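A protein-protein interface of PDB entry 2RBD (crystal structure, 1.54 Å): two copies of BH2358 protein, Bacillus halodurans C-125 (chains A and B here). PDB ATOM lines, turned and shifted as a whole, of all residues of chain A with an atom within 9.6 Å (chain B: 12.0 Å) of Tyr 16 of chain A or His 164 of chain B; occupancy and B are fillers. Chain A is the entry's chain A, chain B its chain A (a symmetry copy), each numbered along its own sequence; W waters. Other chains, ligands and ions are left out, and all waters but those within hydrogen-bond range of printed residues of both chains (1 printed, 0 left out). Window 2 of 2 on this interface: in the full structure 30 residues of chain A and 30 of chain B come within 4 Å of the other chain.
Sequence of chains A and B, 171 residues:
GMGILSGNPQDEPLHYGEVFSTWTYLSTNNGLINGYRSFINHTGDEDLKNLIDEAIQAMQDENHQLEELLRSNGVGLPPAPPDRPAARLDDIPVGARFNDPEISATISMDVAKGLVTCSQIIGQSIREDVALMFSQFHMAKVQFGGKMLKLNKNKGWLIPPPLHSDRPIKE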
ATOM      1  N   PRO A  13      10.087  16.153  40.283  1.00  0.00           N
ATOM      2  CA  PRO A  13      10.079  16.855  39.000  1.00  0.00           C
ATOM      3  C   PRO A  13       8.663  17.124  38.489  1.00  0.00           C
ATOM      4  O   PRO A  13       7.760  16.311  38.670  1.00  0.00           O
ATOM      5  CB  PRO A  13      10.768  15.880  38.049  1.00  0.00           C
ATOM      6  CG  PRO A  13      10.623  14.573  38.654  1.00  0.00           C
ATOM      7  CD  PRO A  13      10.591  14.776  40.148  1.00  0.00           C
ATOM      8  N   LEU A  14       8.498  18.270  37.839  1.00  0.00           N
ATOM      9  CA  LEU A  14       7.313  18.533  37.013  1.00  0.00           C
ATOM     10  C   LEU A  14       7.269  17.570  35.836  1.00  0.00           C
ATOM     11  O   LEU A  14       8.296  17.171  35.293  1.00  0.00           O
ATOM     12  CB  LEU A  14       7.321  19.972  36.479  1.00  0.00           C
ATOM     13  CG  LEU A  14       7.290  21.113  37.522  1.00  0.00           C
ATOM     14  CD1 LEU A  14       7.751  22.425  36.925  1.00  0.00           C
ATOM     15  CD2 LEU A  14       5.885  21.201  38.178  1.00  0.00           C
ATOM     16  N   HIS A  15       6.068  17.194  35.430  1.00  0.00           N
ATOM     17  CA  HIS A  15       5.928  16.471  34.171  1.00  0.00           C
ATOM     18  C   HIS A  15       5.777  17.409  32.983  1.00  0.00           C
ATOM     19  O   HIS A  15       5.630  18.606  33.142  1.00  0.00           O
ATOM     20  CB  HIS A  15       4.858  15.374  34.240  1.00  0.00           C
ATOM     21  CG  HIS A  15       3.433  15.818  34.323  1.00  0.00           C
ATOM     22  ND1 HIS A  15       2.746  16.374  33.257  1.00  0.00           N
ATOM     23  CD2 HIS A  15       2.522  15.641  35.314  1.00  0.00           C
ATOM     24  CE1 HIS A  15       1.484  16.553  33.608  1.00  0.00           C
ATOM     25  NE2 HIS A  15       1.317  16.109  34.844  1.00  0.00           N
ATOM     26  N   TYR A  16       5.950  16.872  31.792  1.00  0.00           N
ATOM     27  CA  TYR A  16       5.933  17.673  30.563  1.00  0.00           C
ATOM     28  C   TYR A  16       4.677  18.497  30.385  1.00  0.00           C
ATOM     29  O   TYR A  16       4.739  19.634  29.919  1.00  0.00           O
ATOM     30  CB  TYR A  16       6.081  16.764  29.360  1.00  0.00           C
ATOM     31  CG  TYR A  16       7.488  16.477  28.862  1.00  0.00           C
ATOM     32  CD1 TYR A  16       8.560  16.380  29.713  1.00  0.00           C
ATOM     33  CD2 TYR A  16       7.692  16.283  27.542  1.00  0.00           C
ATOM     34  CE1 TYR A  16       9.839  16.106  29.223  1.00  0.00           C
ATOM     35  CE2 TYR A  16       8.939  16.020  27.045  1.00  0.00           C
ATOM     36  CZ  TYR A  16      10.008  15.922  27.897  1.00  0.00           C
ATOM     37  OH  TYR A  16      11.271  15.648  27.352  1.00  0.00           O
ATOM     38  N   GLY A  17       3.548  17.936  30.788  1.00  0.00           N
ATOM     39  CA  GLY A  17       2.283  18.663  30.755  1.00  0.00           C
ATOM     40  C   GLY A  17       2.215  19.829  31.702  1.00  0.00           C
ATOM     41  O   GLY A  17       1.725  20.896  31.359  1.00  0.00           O
ATOM     42  N   GLU A  18       2.665  19.623  32.920  1.00  0.00           N
ATOM     43  CA  GLU A  18       2.748  20.696  33.865  1.00  0.00           C
ATOM     44  C   GLU A  18       3.632  21.834  33.363  1.00  0.00           C
ATOM     45  O   GLU A  18       3.281  23.011  33.498  1.00  0.00           O
ATOM     46  CB  GLU A  18       3.266  20.170  35.209  1.00  0.00           C
ATOM     47  CG  GLU A  18       2.213  19.338  35.978  1.00  0.00           C
ATOM     48  CD  GLU A  18       2.776  18.494  37.137  1.00  0.00           C
ATOM     49  OE1 GLU A  18       4.008  18.240  37.229  1.00  0.00           O
ATOM     50  OE2 GLU A  18       1.993  18.129  38.021  1.00  0.00           O
ATOM     51  N   VAL A  19       4.784  21.486  32.797  1.00  0.00           N
ATOM     52  CA  VAL A  19       5.667  22.499  32.250  1.00  0.00           C
ATOM     53  C   VAL A  19       5.000  23.247  31.093  1.00  0.00           C
ATOM     54  O   VAL A  19       4.917  24.489  31.099  1.00  0.00           O
ATOM     55  CB  VAL A  19       7.038  21.904  31.826  1.00  0.00           C
ATOM     56  CG1 VAL A  19       7.892  22.968  31.080  1.00  0.00           C
ATOM     57  CG2 VAL A  19       7.809  21.394  33.090  1.00  0.00           C
ATOM     58  N   PHE A  20       4.485  22.509  30.124  1.00  0.00           N
ATOM     59  CA  PHE A  20       3.904  23.171  28.972  1.00  0.00           C
ATOM     60  C   PHE A  20       2.689  24.017  29.345  1.00  0.00           C
ATOM     61  O   PHE A  20       2.540  25.154  28.874  1.00  0.00           O
ATOM     62  CB  PHE A  20       3.531  22.167  27.877  1.00  0.00           C
ATOM     63  CG  PHE A  20       2.947  22.797  26.666  1.00  0.00           C
ATOM     64  CD1 PHE A  20       3.754  23.423  25.757  1.00  0.00           C
ATOM     65  CD2 PHE A  20       1.590  22.805  26.462  1.00  0.00           C
ATOM     66  CE1 PHE A  20       3.246  24.047  24.635  1.00  0.00           C
ATOM     67  CE2 PHE A  20       1.075  23.418  25.329  1.00  0.00           C
ATOM     68  CZ  PHE A  20       1.893  24.034  24.443  1.00  0.00           C
ATOM     69  N   SER A  21       1.851  23.479  30.204  1.00  0.00           N
ATOM     70  CA  SER A  21       0.624  24.182  30.569  1.00  0.00           C
ATOM     71  C   SER A  21       0.896  25.471  31.356  1.00  0.00           C
ATOM     72  O   SER A  21       0.253  26.496  31.120  1.00  0.00           O
ATOM     73  CB  SER A  21      -0.319  23.272  31.345  1.00  0.00           C
ATOM     74  OG  SER A  21      -0.814  22.283  30.473  1.00  0.00           O
ATOM     75  N   THR A  22       1.802  25.410  32.323  1.00  0.00           N
ATOM     76  CA  THR A  22       2.121  26.574  33.109  1.00  0.00           C
ATOM     77  C   THR A  22       2.858  27.614  32.263  1.00  0.00           C
ATOM     78  O   THR A  22       2.579  28.806  32.363  1.00  0.00           O
ATOM     79  CB  THR A  22       2.909  26.240  34.388  1.00  0.00           C
ATOM     80  OG1 THR A  22       4.146  25.607  34.065  1.00  0.00           O
ATOM     81  CG2 THR A  22       2.068  25.360  35.316  1.00  0.00           C
ATOM     82  N   TRP A  23       3.797  27.169  31.439  1.00  0.00           N
ATOM     83  CA  TRP A  23       4.470  28.082  30.502  1.00  0.00           C
ATOM     84  C   TRP A  23       3.469  28.767  29.579  1.00  0.00           C
ATOM     85  O   TRP A  23       3.524  29.995  29.357  1.00  0.00           O
ATOM     86  CB  TRP A  23       5.491  27.295  29.679  1.00  0.00           C
ATOM     87  CG  TRP A  23       6.321  28.106  28.754  1.00  0.00           C
ATOM     88  CD1 TRP A  23       7.561  28.610  29.014  1.00  0.00           C
ATOM     89  CD2 TRP A  23       6.028  28.457  27.404  1.00  0.00           C
ATOM     90  NE1 TRP A  23       8.041  29.275  27.932  1.00  0.00           N
ATOM     91  CE2 TRP A  23       7.125  29.219  26.925  1.00  0.00           C
ATOM     92  CE3 TRP A  23       4.946  28.218  26.549  1.00  0.00           C
ATOM     93  CZ2 TRP A  23       7.178  29.722  25.641  1.00  0.00           C
ATOM     94  CZ3 TRP A  23       4.988  28.743  25.290  1.00  0.00           C
ATOM     95  CH2 TRP A  23       6.095  29.496  24.847  1.00  0.00           C
ATOM     96  N   THR A  24       2.535  27.996  29.033  1.00  0.00           N
ATOM     97  CA  THR A  24       1.535  28.543  28.163  1.00  0.00           C
ATOM     98  C   THR A  24       0.590  29.541  28.891  1.00  0.00           C
ATOM     99  O   THR A  24       0.230  30.596  28.356  1.00  0.00           O
ATOM    100  CB  THR A  24       0.759  27.401  27.500  1.00  0.00           C
ATOM    101  OG1 THR A  24       1.630  26.664  26.636  1.00  0.00           O
ATOM    102  CG2 THR A  24      -0.383  27.941  26.656  1.00  0.00           C
ATOM    103  N   LEU A  70       8.527  28.300  37.481  1.00  0.00           N
ATOM    104  CA  LEU A  70       9.382  27.978  36.327  1.00  0.00           C
ATOM    105  C   LEU A  70      10.858  28.235  36.570  1.00  0.00           C
ATOM    106  O   LEU A  70      11.698  27.405  36.195  1.00  0.00           O
ATOM    107  CB  LEU A  70       8.905  28.695  35.070  1.00  0.00           C
ATOM    108  CG  LEU A  70       7.507  28.283  34.619  1.00  0.00           C
ATOM    109  CD1 LEU A  70       7.257  28.997  33.291  1.00  0.00           C
ATOM    110  CD2 LEU A  70       7.321  26.787  34.501  1.00  0.00           C
ATOM    111  N   VAL A  75      13.048  26.012  33.816  1.00  0.00           N
ATOM    112  CA  VAL A  75      12.249  26.202  32.609  1.00  0.00           C
ATOM    113  C   VAL A  75      12.412  27.659  32.149  1.00  0.00           C
ATOM    114  O   VAL A  75      12.238  28.586  32.951  1.00  0.00           O
ATOM    115  CB  VAL A  75      10.749  25.899  32.860  1.00  0.00           C
ATOM    116  CG1 VAL A  75       9.932  26.159  31.581  1.00  0.00           C
ATOM    117  CG2 VAL A  75      10.539  24.454  33.440  1.00  0.00           C
ATOM    118  N   GLN A 124      -4.792  17.718  35.192  1.00  0.00           N
ATOM    119  CA  GLN A 124      -3.657  17.011  34.651  1.00  0.00           C
ATOM    120  C   GLN A 124      -2.461  17.028  35.597  1.00  0.00           C
ATOM    121  O   GLN A 124      -1.440  16.395  35.333  1.00  0.00           O
ATOM    122  CB  GLN A 124      -3.290  17.580  33.292  1.00  0.00           C
ATOM    123  CG  GLN A 124      -2.559  18.880  33.325  1.00  0.00           C
ATOM    124  CD  GLN A 124      -1.970  19.229  31.945  1.00  0.00           C
ATOM    125  OE1 GLN A 124      -0.751  19.415  31.809  1.00  0.00           O
ATOM    126  NE2 GLN A 124      -2.840  19.267  30.909  1.00  0.00           N
ATOM    127  N   SER A 125      -2.601  17.735  36.697  1.00  0.00           N
ATOM    128  CA  SER A 125      -1.505  17.878  37.650  1.00  0.00           C
ATOM    129  C   SER A 125      -1.270  16.631  38.484  1.00  0.00           C
ATOM    130  O   SER A 125      -2.191  15.938  38.858  1.00  0.00           O
ATOM    131  CB  SER A 125      -1.760  19.037  38.617  1.00  0.00           C
ATOM    132  OG  SER A 125      -1.614  20.279  37.949  1.00  0.00           O
ATOM    133  N   ILE A 126      -0.005  16.348  38.730  1.00  0.00           N
ATOM    134  CA  ILE A 126       0.429  15.287  39.644  1.00  0.00           C
ATOM    135  C   ILE A 126       1.154  15.896  40.816  1.00  0.00           C
ATOM    136  O   ILE A 126       0.976  15.454  41.944  1.00  0.00           O
ATOM    137  CB  ILE A 126       1.317  14.276  38.915  1.00  0.00           C
ATOM    138  CG1 ILE A 126       0.516  13.563  37.832  1.00  0.00           C
ATOM    139  CG2 ILE A 126       1.899  13.261  39.919  1.00  0.00           C
ATOM    140  CD1 ILE A 126       1.296  12.497  37.044  1.00  0.00           C
ATOM    141  N   ILE B 159       6.779  32.181  19.305  1.00  0.00           N
ATOM    142  CA  ILE B 159       7.612  32.048  20.508  1.00  0.00           C
ATOM    143  C   ILE B 159       7.817  30.553  20.728  1.00  0.00           C
ATOM    144  O   ILE B 159       6.848  29.820  20.828  1.00  0.00           O
ATOM    145  CB  ILE B 159       6.890  32.621  21.730  1.00  0.00           C
ATOM    146  CG1 ILE B 159       6.614  34.117  21.556  1.00  0.00           C
ATOM    147  CG2 ILE B 159       7.721  32.367  22.984  1.00  0.00           C
ATOM    148  CD1 ILE B 159       5.799  34.723  22.722  1.00  0.00           C
ATOM    149  N   PRO B 160       9.069  30.081  20.786  1.00  0.00           N
ATOM    150  CA  PRO B 160       9.255  28.644  20.947  1.00  0.00           C
ATOM    151  C   PRO B 160       8.965  28.181  22.374  1.00  0.00           C
ATOM    152  O   PRO B 160       9.478  28.742  23.293  1.00  0.00           O
ATOM    153  CB  PRO B 160      10.733  28.432  20.624  1.00  0.00           C
ATOM    154  CG  PRO B 160      11.371  29.737  20.900  1.00  0.00           C
ATOM    155  CD  PRO B 160      10.346  30.801  20.652  1.00  0.00           C
ATOM    156  N   PRO B 161       8.133  27.168  22.538  1.00  0.00           N
ATOM    157  CA  PRO B 161       7.916  26.588  23.853  1.00  0.00           C
ATOM    158  C   PRO B 161       9.052  25.663  24.245  1.00  0.00           C
ATOM    159  O   PRO B 161       9.933  25.387  23.437  1.00  0.00           O
ATOM    160  CB  PRO B 161       6.618  25.804  23.678  1.00  0.00           C
ATOM    161  CG  PRO B 161       6.527  25.547  22.275  1.00  0.00           C
ATOM    162  CD  PRO B 161       7.299  26.528  21.518  1.00  0.00           C
ATOM    163  N   PRO B 162       9.030  25.184  25.481  1.00  0.00           N
ATOM    164  CA  PRO B 162      10.047  24.203  25.879  1.00  0.00           C
ATOM    165  C   PRO B 162      10.072  23.001  24.943  1.00  0.00           C
ATOM    166  O   PRO B 162       9.027  22.475  24.596  1.00  0.00           O
ATOM    167  CB  PRO B 162       9.651  23.781  27.295  1.00  0.00           C
ATOM    168  CG  PRO B 162       8.396  24.551  27.630  1.00  0.00           C
ATOM    169  CD  PRO B 162       8.090  25.533  26.556  1.00  0.00           C
ATOM    170  N   LEU B 163      11.265  22.565  24.542  1.00  0.00           N
ATOM    171  CA  LEU B 163      11.402  21.536  23.524  1.00  0.00           C
ATOM    172  C   LEU B 163      11.918  20.260  24.119  1.00  0.00           C
ATOM    173  O   LEU B 163      12.740  20.275  25.021  1.00  0.00           O
ATOM    174  CB  LEU B 163      12.363  22.011  22.420  1.00  0.00           C
ATOM    175  CG  LEU B 163      11.962  23.292  21.698  1.00  0.00           C
ATOM    176  CD1 LEU B 163      13.035  23.760  20.717  1.00  0.00           C
ATOM    177  CD2 LEU B 163      10.631  23.065  20.962  1.00  0.00           C
ATOM    178  N   HIS B 164      11.442  19.147  23.606  1.00  0.00           N
ATOM    179  CA  HIS B 164      11.891  17.838  24.013  1.00  0.00           C
ATOM    180  C   HIS B 164      13.285  17.589  23.396  1.00  0.00           C
ATOM    181  O   HIS B 164      13.492  17.917  22.229  1.00  0.00           O
ATOM    182  CB  HIS B 164      10.905  16.803  23.471  1.00  0.00           C
ATOM    183  CG  HIS B 164      11.360  15.403  23.617  1.00  0.00           C
ATOM    184  ND1 HIS B 164      11.531  14.797  24.837  1.00  0.00           N
ATOM    185  CD2 HIS B 164      11.675  14.483  22.678  1.00  0.00           C
ATOM    186  CE1 HIS B 164      11.925  13.554  24.637  1.00  0.00           C
ATOM    187  NE2 HIS B 164      12.011  13.340  23.334  1.00  0.00           N
ATOM    188  N   SER B 165      14.203  17.037  24.172  1.00  0.00           N
ATOM    189  CA  SER B 165      15.523  16.617  23.658  1.00  0.00           C
ATOM    190  C   SER B 165      15.504  15.115  23.431  1.00  0.00           C
ATOM    191  O   SER B 165      15.326  14.371  24.384  1.00  0.00           O
ATOM    192  CB  SER B 165      16.617  16.943  24.680  1.00  0.00           C
ATOM    193  OG  SER B 165      16.734  18.342  24.902  1.00  0.00           O
ATOM    194  N   ASP B 166      15.683  14.674  22.182  1.00  0.00           N
ATOM    195  CA  ASP B 166      15.664  13.235  21.841  1.00  0.00           C
ATOM    196  C   ASP B 166      17.080  12.633  21.957  1.00  0.00           C
ATOM    197  O   ASP B 166      17.540  12.273  23.056  1.00  0.00           O
ATOM    198  CB  ASP B 166      15.101  13.010  20.423  1.00  0.00           C
HETATM  199  O   HOH W   1      13.759  16.882  27.140  1.00  0.00           O
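O of Phe 20 of chain A is in hydrogen-bond range of OG1 of Thr 24 of chain A (2.8 Å).
OG1 of Thr 22 of chain A is in hydrogen-bond range of O of Val 19 of chain A (3.3 Å).
ND1 of His 164 of chain B sits at hydrogen-bond distance from OH of Tyr 16 of chain A (2.7 Å).
Of the 8 printed residues of chain B, 5 touch a printed residue of chain A.
Printed residues of chain B that touch a printed residue of chain A: Ile 159, Pro 160, Pro 161, Pro 162 and His 164.
Hydrophobic or aromatic side chains of chain B that line the printed part of chain A: Ile 159, Pro 161, Pro 162 and His 164.
Hydrophobic or aromatic side chains of chain A that line the printed part of chain B: Tyr 16, Val 19, Phe 20 and Trp 23.
Among the printed residues, no Asp or Glu carboxylate lies within 4 Å of a Lys or Arg side-chain nitrogen of the other chain.
Tyr 16 of chain A touches just one residue of chain B: His 164 (2.7 Å).
His 164 of chain B touches just one residue of chain A: Tyr 16 (2.7 Å).
No residue of chain B comes within 4 Å of Leu 14 of chain A.
No residue of chain B comes within 4 Å of His 15 of chain A.
No residue of chain B comes within 4 Å of Gly 17 of chain A.
No residue of chain B comes within 4 Å of Glu 18 of chain A.
Of chain B, only Pro 162 comes within 4 Å of Val 19 of chain A.
Of chain B, only Pro 161 comes within 4 Å of Phe 20 of chain A.
Of the printed residues of chain B, Trp 23 of chain A touches Ile 159 (3.8 Å), Pro 160 (3.4 Å), Pro 161 (3.6 Å) and Pro 162 (3.7 Å).
Of the printed residues of chain A, Pro 160 of chain B touches Trp 23 (3.4 Å).
Of the printed residues of chain A, Pro 161 of chain B touches Phe 20 and Trp 23.
The nearest printed residue of chain B that does not touch Tyr 16 of chain A is Ser 165 of chain B (4.5 Å).
The nearest printed residue of chain A that does not touch Ile 159 of chain B is Phe 20 of chain A (7.8 Å).
Water W1 lies within hydrogen-bond range of the side-chain hydroxyl (OH) of Tyr 16 of chain A and the backbone NH (N) of Ser 165 of chain B.
No position is printed for both chains.
Of the 7 pairs that touch across the chains among the printed residues, none has its exchanged pair printed and touching as well.
Among the printed residues, merely in contact across the chains: Trp 23 of chain A with Pro 160 of chain B (3.4 Å), Trp 23 of chain A with Pro 161 of chain B (3.6 Å), Trp 23 of chain A with Pro 162 of chain B (3.7 Å), Trp 23 of chain A with Ile 159 of chain B (3.8 Å), Val 19 of chain A with Pro 162 of chain B (3.8 Å) and Phe 20 of chain A with Pro 161 of chain B (3.9 Å).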
